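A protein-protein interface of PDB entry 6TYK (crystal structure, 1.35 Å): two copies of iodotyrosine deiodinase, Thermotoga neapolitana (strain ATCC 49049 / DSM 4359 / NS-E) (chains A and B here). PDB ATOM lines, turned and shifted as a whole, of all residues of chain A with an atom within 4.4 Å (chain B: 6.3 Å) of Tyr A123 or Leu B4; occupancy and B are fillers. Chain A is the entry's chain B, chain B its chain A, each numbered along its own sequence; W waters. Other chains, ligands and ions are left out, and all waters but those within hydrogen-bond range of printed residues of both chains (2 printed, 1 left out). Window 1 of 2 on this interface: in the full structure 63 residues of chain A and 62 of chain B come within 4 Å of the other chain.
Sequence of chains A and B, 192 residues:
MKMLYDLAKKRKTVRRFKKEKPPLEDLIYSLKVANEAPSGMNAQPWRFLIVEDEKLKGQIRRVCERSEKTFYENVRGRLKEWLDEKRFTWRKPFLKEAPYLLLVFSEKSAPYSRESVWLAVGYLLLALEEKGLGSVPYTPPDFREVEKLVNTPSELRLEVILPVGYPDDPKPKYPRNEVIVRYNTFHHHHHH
Printed residues of chain B that touch a printed residue of chain A: Met B3, Leu B4, Tyr B5, Ala B8, Lys B9, Arg B11, Leu B119, Val B121, Gly B122, Tyr B123, Leu B125 and Leu B126. Printed residues of chain A that touch a printed residue of chain B: Leu A4, Tyr A29, Val A33, Glu A36, Pro A38, Leu A119, Val A121, Gly A122, Tyr A123, Leu A125, Leu A126, Ala A127 and Glu A130. Among the printed residues, no Asp or Glu carboxylate lies within 4 Å of a Lys or Arg side-chain nitrogen of the other chain.
Water W2 bridges OE2 of Glu A130 (2.7 Å) and SD of Met B3 (3.7 Å). Water W1 lies within hydrogen-bond range of the side-chain carboxylate of Glu A36 and the side-chain amino group of Lys B9.
The side-chain hydroxyl (OH) of Tyr A29 is in hydrogen-bond range of the backbone NH (N) of Tyr B5. The backbone NH (N) of Leu B4 is in hydrogen-bond range of the side-chain carboxylate (OE2) of Glu A130 (2.8 Å). The backbone NH (N) of Leu B4 is in hydrogen-bond range of the side-chain hydroxyl (OH) of Tyr A29, 3.5 Å away.
CA of Lys B9 touches OE1 of Glu A36, at 3.5 Å. Pro A38 touches Arg B11. Leu B125 touches Pro A38 (CD1 to CG, 3.7 Å). CG1 of Val B121 touches CD1 of Leu A119, 3.97 Å away. Val A121 touches Leu B119. Gly A122 touches Leu B119 (CA to O, 3.7 Å). CE2 of Tyr A123 touches CB of Ala B8, at 3.7 Å. Tyr A123 touches Arg B11 (OH to CD, 3.7 Å). CD1 of Leu B126 touches CD1 of Tyr A123 (3.6 Å). Leu A126 touches Leu B126.
Of chain B, only Leu B4, Ala B8, Arg B11, Gly B122 and Leu B126 come within 4 Å of Tyr A123. Leu B4 touches just these residues of chain A: Tyr A29, Val A33, Tyr A123, Leu A126, Ala A127 and Glu A130. Of the printed residues of chain A, Lys B9 touches Glu A36. Of the printed residues of chain B, Glu A36 touches Tyr B5, Ala B8 and Lys B9. Printed residues of chain A within 4 Å of Gly B122: Leu A119 and Tyr A123. Leu B7 touches none of the printed residues of chain A. The nearest printed residue of chain B that does not touch Val A121 is Tyr B123 (5.6 Å).
The side-chain hydroxyl (OH) of Tyr A29 is in hydrogen-bond range of the side-chain carboxylate (OE1) of Glu A130 (2.5 Å). The side-chain carboxylate (OD2) of Asp B6 lies within hydrogen-bond range of the backbone NH (N) of Met B3, 3.1 Å away.
Leu A4 touches Leu B126, and with the chains exchanged Leu A126 touches Leu B4. Leu A119 touches Gly B122, and with the chains exchanged Gly A122 touches Leu B119. Tyr A123 touches Leu B126, and with the chains exchanged Leu A126 touches Tyr B123. Leu A126 touches its own counterpart, Leu B126. Of the 30 pairs that touch across the chains among the printed residues, 13 have their exchanged pair printed and touching as well.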
ATOM      1  N   LEU A   4     -12.759 -21.059 -12.339  1.00  0.00           N
ATOM      2  CA  LEU A   4     -11.896 -20.188 -11.552  1.00  0.00           C
ATOM      3  C   LEU A   4     -12.715 -19.277 -10.638  1.00  0.00           C
ATOM      4  O   LEU A   4     -12.347 -19.047  -9.486  1.00  0.00           O
ATOM      5  CB  LEU A   4     -10.990 -19.356 -12.458  1.00  0.00           C
ATOM      6  CG  LEU A   4      -9.992 -18.469 -11.718  1.00  0.00           C
ATOM      7  CD1 LEU A   4      -8.958 -19.304 -10.980  1.00  0.00           C
ATOM      8  CD2 LEU A   4      -9.307 -17.509 -12.673  1.00  0.00           C
ATOM      9  N   TYR A  29       2.866 -28.029  -4.274  1.00  0.00           N
ATOM     10  CA  TYR A  29       2.059 -27.775  -5.463  1.00  0.00           C
ATOM     11  C   TYR A  29       1.684 -26.291  -5.550  1.00  0.00           C
ATOM     12  O   TYR A  29       1.819 -25.660  -6.597  1.00  0.00           O
ATOM     13  CB  TYR A  29       0.788 -28.634  -5.448  1.00  0.00           C
ATOM     14  CG  TYR A  29      -0.235 -28.222  -6.486  1.00  0.00           C
ATOM     15  CD1 TYR A  29      -0.150 -28.694  -7.787  1.00  0.00           C
ATOM     16  CD2 TYR A  29      -1.270 -27.352  -6.168  1.00  0.00           C
ATOM     17  CE1 TYR A  29      -1.069 -28.328  -8.740  1.00  0.00           C
ATOM     18  CE2 TYR A  29      -2.202 -26.976  -7.119  1.00  0.00           C
ATOM     19  CZ  TYR A  29      -2.090 -27.468  -8.405  1.00  0.00           C
ATOM     20  OH  TYR A  29      -3.002 -27.102  -9.362  1.00  0.00           O
ATOM     21  N   VAL A  33       2.606 -23.545  -8.442  1.00  0.00           N
ATOM     22  CA  VAL A  33       1.633 -22.714  -9.137  1.00  0.00           C
ATOM     23  C   VAL A  33       2.066 -21.257  -9.045  1.00  0.00           C
ATOM     24  O   VAL A  33       2.119 -20.545 -10.054  1.00  0.00           O
ATOM     25  CB  VAL A  33       0.217 -22.882  -8.557  1.00  0.00           C
ATOM     26  CG1 VAL A  33      -0.724 -21.870  -9.167  1.00  0.00           C
ATOM     27  CG2 VAL A  33      -0.296 -24.292  -8.814  1.00  0.00           C
ATOM     28  N   ALA A  34       2.402 -20.814  -7.837  1.00  0.00           N
ATOM     29  CA  ALA A  34       2.787 -19.420  -7.636  1.00  0.00           C
ATOM     30  C   ALA A  34       4.028 -19.066  -8.460  1.00  0.00           C
ATOM     31  O   ALA A  34       4.139 -17.955  -8.976  1.00  0.00           O
ATOM     32  CB  ALA A  34       3.036 -19.145  -6.166  1.00  0.00           C
ATOM     33  N   GLU A  36       4.825 -19.953 -11.298  1.00  0.00           N
ATOM     34  CA  GLU A  36       4.483 -19.727 -12.702  1.00  0.00           C
ATOM     35  C   GLU A  36       3.975 -18.312 -12.957  1.00  0.00           C
ATOM     36  O   GLU A  36       3.779 -17.915 -14.104  1.00  0.00           O
ATOM     37  CB  GLU A  36       3.426 -20.738 -13.161  1.00  0.00           C
ATOM     38  CG  GLU A  36       3.937 -22.148 -13.308  1.00  0.00           C
ATOM     39  CD  GLU A  36       5.027 -22.244 -14.356  1.00  0.00           C
ATOM     40  OE1 GLU A  36       4.958 -21.496 -15.367  1.00  0.00           O
ATOM     41  OE2 GLU A  36       5.959 -23.053 -14.168  1.00  0.00           O
ATOM     42  N   ALA A  37       3.739 -17.566 -11.892  1.00  0.00           N
ATOM     43  CA  ALA A  37       3.267 -16.196 -12.016  1.00  0.00           C
ATOM     44  C   ALA A  37       4.284 -15.309 -12.731  1.00  0.00           C
ATOM     45  O   ALA A  37       5.488 -15.585 -12.728  1.00  0.00           O
ATOM     46  CB  ALA A  37       2.945 -15.623 -10.650  1.00  0.00           C
ATOM     47  N   PRO A  38       3.807 -14.226 -13.344  1.00  0.00           N
ATOM     48  CA  PRO A  38       4.698 -13.203 -13.889  1.00  0.00           C
ATOM     49  C   PRO A  38       5.412 -12.441 -12.782  1.00  0.00           C
ATOM     50  O   PRO A  38       5.016 -12.519 -11.616  1.00  0.00           O
ATOM     51  CB  PRO A  38       3.737 -12.280 -14.628  1.00  0.00           C
ATOM     52  CG  PRO A  38       2.462 -12.397 -13.862  1.00  0.00           C
ATOM     53  CD  PRO A  38       2.387 -13.857 -13.491  1.00  0.00           C
ATOM     54  N   LEU A 119       1.401 -10.502  -6.198  1.00  0.00           N
ATOM     55  CA  LEU A 119       0.690 -11.100  -7.310  1.00  0.00           C
ATOM     56  C   LEU A 119       0.793 -12.638  -7.208  1.00  0.00           C
ATOM     57  O   LEU A 119      -0.209 -13.351  -7.318  1.00  0.00           O
ATOM     58  CB  LEU A 119       1.293 -10.573  -8.607  1.00  0.00           C
ATOM     59  CG  LEU A 119       0.601 -10.881  -9.925  1.00  0.00           C
ATOM     60  CD1 LEU A 119       1.099  -9.914 -10.999  1.00  0.00           C
ATOM     61  CD2 LEU A 119       0.841 -12.328 -10.364  1.00  0.00           C
ATOM     62  N   ALA A 120       2.010 -13.150  -7.007  1.00  0.00           N
ATOM     63  CA  ALA A 120       2.205 -14.585  -6.849  1.00  0.00           C
ATOM     64  C   ALA A 120       1.446 -15.151  -5.635  1.00  0.00           C
ATOM     65  O   ALA A 120       0.991 -16.296  -5.670  1.00  0.00           O
ATOM     66  CB  ALA A 120       3.689 -14.905  -6.746  1.00  0.00           C
ATOM     67  N   VAL A 121       1.300 -14.363  -4.572  1.00  0.00           N
ATOM     68  CA  VAL A 121       0.528 -14.816  -3.415  1.00  0.00           C
ATOM     69  C   VAL A 121      -0.932 -15.054  -3.826  1.00  0.00           C
ATOM     70  O   VAL A 121      -1.577 -15.977  -3.330  1.00  0.00           O
ATOM     71  CB  VAL A 121       0.629 -13.828  -2.242  1.00  0.00           C
ATOM     72  CG1 VAL A 121      -0.438 -14.121  -1.184  1.00  0.00           C
ATOM     73  CG2 VAL A 121       2.027 -13.881  -1.629  1.00  0.00           C
ATOM     74  N   GLY A 122      -1.436 -14.255  -4.761  1.00  0.00           N
ATOM     75  CA  GLY A 122      -2.772 -14.477  -5.293  1.00  0.00           C
ATOM     76  C   GLY A 122      -2.883 -15.866  -5.914  1.00  0.00           C
ATOM     77  O   GLY A 122      -3.826 -16.619  -5.632  1.00  0.00           O
ATOM     78  N   TYR A 123      -1.917 -16.218  -6.759  1.00  0.00           N
ATOM     79  CA  TYR A 123      -1.870 -17.560  -7.338  1.00  0.00           C
ATOM     80  C   TYR A 123      -1.829 -18.613  -6.247  1.00  0.00           C
ATOM     81  O   TYR A 123      -2.534 -19.614  -6.310  1.00  0.00           O
ATOM     82  CB  TYR A 123      -0.605 -17.739  -8.167  1.00  0.00           C
ATOM     83  CG  TYR A 123      -0.625 -17.207  -9.586  1.00  0.00           C
ATOM     84  CD1 TYR A 123      -1.221 -15.990  -9.904  1.00  0.00           C
ATOM     85  CD2 TYR A 123       0.030 -17.898 -10.603  1.00  0.00           C
ATOM     86  CE1 TYR A 123      -1.196 -15.502 -11.204  1.00  0.00           C
ATOM     87  CE2 TYR A 123       0.062 -17.431 -11.885  1.00  0.00           C
ATOM     88  CZ  TYR A 123      -0.552 -16.230 -12.189  1.00  0.00           C
ATOM     89  OH  TYR A 123      -0.503 -15.780 -13.488  1.00  0.00           O
ATOM     90  N   LEU A 124      -0.969 -18.379  -5.263  1.00  0.00           N
ATOM     91  CA  LEU A 124      -0.723 -19.314  -4.183  1.00  0.00           C
ATOM     92  C   LEU A 124      -2.000 -19.616  -3.414  1.00  0.00           C
ATOM     93  O   LEU A 124      -2.321 -20.776  -3.158  1.00  0.00           O
ATOM     94  CB  LEU A 124       0.343 -18.734  -3.255  1.00  0.00           C
ATOM     95  CG  LEU A 124       1.120 -19.685  -2.345  1.00  0.00           C
ATOM     96  CD1 LEU A 124       2.286 -18.926  -1.732  1.00  0.00           C
ATOM     97  CD2 LEU A 124       0.236 -20.256  -1.267  1.00  0.00           C
ATOM     98  N   LEU A 125      -2.740 -18.571  -3.043  1.00  0.00           N
ATOM     99  CA  LEU A 125      -3.957 -18.749  -2.263  1.00  0.00           C
ATOM    100  C   LEU A 125      -5.000 -19.546  -3.031  1.00  0.00           C
ATOM    101  O   LEU A 125      -5.714 -20.359  -2.448  1.00  0.00           O
ATOM    102  CB  LEU A 125      -4.534 -17.400  -1.855  1.00  0.00           C
ATOM    103  CG  LEU A 125      -3.672 -16.581  -0.901  1.00  0.00           C
ATOM    104  CD1 LEU A 125      -4.414 -15.327  -0.484  1.00  0.00           C
ATOM    105  CD2 LEU A 125      -3.318 -17.421   0.318  1.00  0.00           C
ATOM    106  N   LEU A 126      -5.100 -19.311  -4.336  1.00  0.00           N
ATOM    107  CA  LEU A 126      -6.040 -20.071  -5.154  1.00  0.00           C
ATOM    108  C   LEU A 126      -5.626 -21.537  -5.227  1.00  0.00           C
ATOM    109  O   LEU A 126      -6.467 -22.432  -5.203  1.00  0.00           O
ATOM    110  CB  LEU A 126      -6.151 -19.471  -6.551  1.00  0.00           C
ATOM    111  CG  LEU A 126      -6.880 -18.133  -6.597  1.00  0.00           C
ATOM    112  CD1 LEU A 126      -6.679 -17.498  -7.957  1.00  0.00           C
ATOM    113  CD2 LEU A 126      -8.362 -18.341  -6.319  1.00  0.00           C
ATOM    114  N   ALA A 127      -4.323 -21.781  -5.314  1.00  0.00           N
ATOM    115  CA  ALA A 127      -3.806 -23.141  -5.361  1.00  0.00           C
ATOM    116  C   ALA A 127      -4.091 -23.882  -4.058  1.00  0.00           C
ATOM    117  O   ALA A 127      -4.471 -25.049  -4.077  1.00  0.00           O
ATOM    118  CB  ALA A 127      -2.312 -23.132  -5.661  1.00  0.00           C
ATOM    119  N   GLU A 130      -7.611 -24.874  -4.099  1.00  0.00           N
ATOM    120  CA  GLU A 130      -7.786 -26.022  -4.980  1.00  0.00           C
ATOM    121  C   GLU A 130      -7.444 -27.331  -4.265  1.00  0.00           C
ATOM    122  O   GLU A 130      -8.088 -28.367  -4.481  1.00  0.00           O
ATOM    123  CB  GLU A 130      -6.920 -25.867  -6.227  1.00  0.00           C
ATOM    124  CG  GLU A 130      -7.171 -26.918  -7.283  1.00  0.00           C
ATOM    125  CD  GLU A 130      -6.202 -26.816  -8.434  1.00  0.00           C
ATOM    126  OE1 GLU A 130      -5.046 -26.426  -8.188  1.00  0.00           O
ATOM    127  OE2 GLU A 130      -6.596 -27.122  -9.579  1.00  0.00           O
ATOM    128  N   LYS B   2      -7.437 -30.921 -15.958  1.00  0.00           N
ATOM    129  CA  LYS B   2      -7.454 -29.487 -15.692  1.00  0.00           C
ATOM    130  C   LYS B   2      -7.051 -29.166 -14.256  1.00  0.00           C
ATOM    131  O   LYS B   2      -7.781 -29.476 -13.316  1.00  0.00           O
ATOM    132  CB  LYS B   2      -8.841 -28.904 -15.973  1.00  0.00           C
ATOM    133  CG  LYS B   2      -9.267 -28.954 -17.431  1.00  0.00           C
ATOM    134  CD  LYS B   2     -10.583 -28.219 -17.632  1.00  0.00           C
ATOM    135  CE  LYS B   2     -10.947 -28.118 -19.104  1.00  0.00           C
ATOM    136  NZ  LYS B   2     -12.193 -27.328 -19.307  1.00  0.00           N
ATOM    137  N   MET B   3      -5.888 -28.544 -14.095  1.00  0.00           N
ATOM    138  CA  MET B   3      -5.452 -28.066 -12.789  1.00  0.00           C
ATOM    139  C   MET B   3      -5.162 -26.574 -12.875  1.00  0.00           C
ATOM    140  O   MET B   3      -4.886 -26.048 -13.955  1.00  0.00           O
ATOM    141  CB  MET B   3      -4.195 -28.808 -12.325  1.00  0.00           C
ATOM    142  CG  MET B   3      -4.369 -30.308 -12.133  1.00  0.00           C
ATOM    143  SD  MET B   3      -5.467 -30.743 -10.768  1.00  0.00           S
ATOM    144  CE  MET B   3      -4.627 -29.974  -9.383  1.00  0.00           C
ATOM    145  N   LEU B   4      -5.228 -25.892 -11.736  1.00  0.00           N
ATOM    146  CA  LEU B   4      -4.843 -24.491 -11.680  1.00  0.00           C
ATOM    147  C   LEU B   4      -3.409 -24.342 -12.174  1.00  0.00           C
ATOM    148  O   LEU B   4      -3.066 -23.365 -12.837  1.00  0.00           O
ATOM    149  CB  LEU B   4      -4.958 -23.964 -10.253  1.00  0.00           C
ATOM    150  CG  LEU B   4      -4.635 -22.480 -10.079  1.00  0.00           C
ATOM    151  CD1 LEU B   4      -5.678 -21.624 -10.786  1.00  0.00           C
ATOM    152  CD2 LEU B   4      -4.552 -22.123  -8.606  1.00  0.00           C
ATOM    153  N   TYR B   5      -2.571 -25.322 -11.854  1.00  0.00           N
ATOM    154  CA  TYR B   5      -1.191 -25.299 -12.310  1.00  0.00           C
ATOM    155  C   TYR B   5      -1.104 -25.168 -13.825  1.00  0.00           C
ATOM    156  O   TYR B   5      -0.281 -24.422 -14.336  1.00  0.00           O
ATOM    157  CB  TYR B   5      -0.423 -26.548 -11.861  1.00  0.00           C
ATOM    158  CG  TYR B   5       0.988 -26.556 -12.400  1.00  0.00           C
ATOM    159  CD1 TYR B   5       1.983 -25.801 -11.795  1.00  0.00           C
ATOM    160  CD2 TYR B   5       1.317 -27.287 -13.537  1.00  0.00           C
ATOM    161  CE1 TYR B   5       3.270 -25.786 -12.290  1.00  0.00           C
ATOM    162  CE2 TYR B   5       2.605 -27.275 -14.045  1.00  0.00           C
ATOM    163  CZ  TYR B   5       3.579 -26.524 -13.413  1.00  0.00           C
ATOM    164  OH  TYR B   5       4.865 -26.505 -13.906  1.00  0.00           O
ATOM    165  N   ASP B   6      -1.948 -25.904 -14.543  1.00  0.00           N
ATOM    166  CA  ASP B   6      -1.927 -25.861 -15.998  1.00  0.00           C
ATOM    167  C   ASP B   6      -2.292 -24.468 -16.505  1.00  0.00           C
ATOM    168  O   ASP B   6      -1.733 -23.981 -17.484  1.00  0.00           O
ATOM    169  CB  ASP B   6      -2.874 -26.915 -16.566  1.00  0.00           C
ATOM    170  CG  ASP B   6      -2.469 -28.323 -16.178  1.00  0.00           C
ATOM    171  OD1 ASP B   6      -1.263 -28.645 -16.279  1.00  0.00           O
ATOM    172  OD2 ASP B   6      -3.350 -29.106 -15.762  1.00  0.00           O
ATOM    173  N   LEU B   7      -3.226 -23.820 -15.823  1.00  0.00           N
ATOM    174  CA  LEU B   7      -3.648 -22.479 -16.211  1.00  0.00           C
ATOM    175  C   LEU B   7      -2.515 -21.485 -15.959  1.00  0.00           C
ATOM    176  O   LEU B   7      -2.170 -20.669 -16.824  1.00  0.00           O
ATOM    177  CB  LEU B   7      -4.879 -22.076 -15.409  1.00  0.00           C
ATOM    178  CG  LEU B   7      -5.529 -20.741 -15.768  1.00  0.00           C
ATOM    179  CD1 LEU B   7      -6.189 -20.808 -17.149  1.00  0.00           C
ATOM    180  CD2 LEU B   7      -6.534 -20.366 -14.696  1.00  0.00           C
ATOM    181  N   ALA B   8      -1.934 -21.560 -14.765  1.00  0.00           N
ATOM    182  CA  ALA B   8      -0.800 -20.710 -14.411  1.00  0.00           C
ATOM    183  C   ALA B   8       0.386 -20.948 -15.341  1.00  0.00           C
ATOM    184  O   ALA B   8       1.068 -20.010 -15.756  1.00  0.00           O
ATOM    185  CB  ALA B   8      -0.392 -20.944 -12.960  1.00  0.00           C
ATOM    186  N   LYS B   9       0.633 -22.212 -15.670  1.00  0.00           N
ATOM    187  CA  LYS B   9       1.770 -22.541 -16.508  1.00  0.00           C
ATOM    188  C   LYS B   9       1.599 -21.962 -17.906  1.00  0.00           C
ATOM    189  O   LYS B   9       2.543 -21.417 -18.481  1.00  0.00           O
ATOM    190  CB  LYS B   9       1.974 -24.056 -16.576  1.00  0.00           C
ATOM    191  CG  LYS B   9       3.289 -24.431 -17.238  1.00  0.00           C
ATOM    192  CD  LYS B   9       3.485 -25.926 -17.344  1.00  0.00           C
ATOM    193  CE  LYS B   9       4.937 -26.243 -17.695  1.00  0.00           C
ATOM    194  NZ  LYS B   9       5.593 -25.122 -18.436  1.00  0.00           N
ATOM    195  N   ARG B  11      -0.307 -19.421 -18.888  1.00  0.00           N
ATOM    196  CA  ARG B  11      -0.443 -17.972 -18.934  1.00  0.00           C
ATOM    197  C   ARG B  11       0.928 -17.318 -19.082  1.00  0.00           C
ATOM    198  O   ARG B  11       1.874 -17.652 -18.369  1.00  0.00           O
ATOM    199  CB  ARG B  11      -1.173 -17.461 -17.689  1.00  0.00           C
ATOM    200  CG  ARG B  11      -1.619 -16.016 -17.787  1.00  0.00           C
ATOM    201  CD  ARG B  11      -0.659 -15.076 -17.077  1.00  0.00           C
ATOM    202  NE  ARG B  11      -0.843 -13.701 -17.525  1.00  0.00           N
ATOM    203  CZ  ARG B  11       0.160 -12.843 -17.682  1.00  0.00           C
ATOM    204  NH1 ARG B  11       1.394 -13.221 -17.393  1.00  0.00           N
ATOM    205  NH2 ARG B  11      -0.068 -11.613 -18.114  1.00  0.00           N
ATOM    206  N   LEU B 119      -2.282  -8.726  -5.093  1.00  0.00           N
ATOM    207  CA  LEU B 119      -2.815 -10.069  -4.904  1.00  0.00           C
ATOM    208  C   LEU B 119      -4.018 -10.280  -5.838  1.00  0.00           C
ATOM    209  O   LEU B 119      -4.104 -11.279  -6.559  1.00  0.00           O
ATOM    210  CB  LEU B 119      -3.212 -10.228  -3.448  1.00  0.00           C
ATOM    211  CG  LEU B 119      -3.547 -11.621  -2.941  1.00  0.00           C
ATOM    212  CD1 LEU B 119      -3.459 -11.621  -1.428  1.00  0.00           C
ATOM    213  CD2 LEU B 119      -4.929 -12.033  -3.382  1.00  0.00           C
ATOM    214  N   VAL B 121      -4.642  -8.681  -8.536  1.00  0.00           N
ATOM    215  CA  VAL B 121      -4.156  -8.715  -9.912  1.00  0.00           C
ATOM    216  C   VAL B 121      -3.750 -10.141 -10.321  1.00  0.00           C
ATOM    217  O   VAL B 121      -3.978 -10.563 -11.454  1.00  0.00           O
ATOM    218  CB  VAL B 121      -3.010  -7.712 -10.141  1.00  0.00           C
ATOM    219  CG1 VAL B 121      -2.329  -7.976 -11.494  1.00  0.00           C
ATOM    220  CG2 VAL B 121      -3.518  -6.287 -10.061  1.00  0.00           C
ATOM    221  N   GLY B 122      -3.195 -10.897  -9.385  1.00  0.00           N
ATOM    222  CA  GLY B 122      -2.905 -12.300  -9.641  1.00  0.00           C
ATOM    223  C   GLY B 122      -4.154 -13.077 -10.017  1.00  0.00           C
ATOM    224  O   GLY B 122      -4.149 -13.816 -10.997  1.00  0.00           O
ATOM    225  N   TYR B 123      -5.236 -12.889  -9.254  1.00  0.00           N
ATOM    226  CA  TYR B 123      -6.516 -13.500  -9.602  1.00  0.00           C
ATOM    227  C   TYR B 123      -6.931 -13.059 -11.000  1.00  0.00           C
ATOM    228  O   TYR B 123      -7.355 -13.860 -11.829  1.00  0.00           O
ATOM    229  CB  TYR B 123      -7.613 -13.050  -8.641  1.00  0.00           C
ATOM    230  CG  TYR B 123      -7.715 -13.764  -7.309  1.00  0.00           C
ATOM    231  CD1 TYR B 123      -6.590 -14.158  -6.596  1.00  0.00           C
ATOM    232  CD2 TYR B 123      -8.963 -14.000  -6.748  1.00  0.00           C
ATOM    233  CE1 TYR B 123      -6.709 -14.787  -5.370  1.00  0.00           C
ATOM    234  CE2 TYR B 123      -9.097 -14.623  -5.517  1.00  0.00           C
ATOM    235  CZ  TYR B 123      -7.968 -15.019  -4.838  1.00  0.00           C
ATOM    236  OH  TYR B 123      -8.080 -15.642  -3.620  1.00  0.00           O
ATOM    237  N   LEU B 125      -5.299 -11.907 -13.617  1.00  0.00           N
ATOM    238  CA  LEU B 125      -4.554 -12.451 -14.751  1.00  0.00           C
ATOM    239  C   LEU B 125      -4.948 -13.890 -15.061  1.00  0.00           C
ATOM    240  O   LEU B 125      -5.027 -14.277 -16.228  1.00  0.00           O
ATOM    241  CB  LEU B 125      -3.052 -12.378 -14.503  1.00  0.00           C
ATOM    242  CG  LEU B 125      -2.484 -10.972 -14.317  1.00  0.00           C
ATOM    243  CD1 LEU B 125      -0.966 -11.051 -14.181  1.00  0.00           C
ATOM    244  CD2 LEU B 125      -2.871 -10.064 -15.474  1.00  0.00           C
ATOM    245  N   LEU B 126      -5.170 -14.690 -14.024  1.00  0.00           N
ATOM    246  CA  LEU B 126      -5.638 -16.054 -14.243  1.00  0.00           C
ATOM    247  C   LEU B 126      -7.021 -16.074 -14.886  1.00  0.00           C
ATOM    248  O   LEU B 126      -7.293 -16.891 -15.766  1.00  0.00           O
ATOM    249  CB  LEU B 126      -5.625 -16.845 -12.934  1.00  0.00           C
ATOM    250  CG  LEU B 126      -4.219 -17.134 -12.417  1.00  0.00           C
ATOM    251  CD1 LEU B 126      -4.261 -17.645 -10.983  1.00  0.00           C
ATOM    252  CD2 LEU B 126      -3.516 -18.116 -13.329  1.00  0.00           C
HETATM  253  O   HOH W   1       6.855 -22.545 -17.112  1.00  0.00           O
HETATM  254  O   HOH W   2      -8.584 -28.877  -9.927  1.00  0.00           O
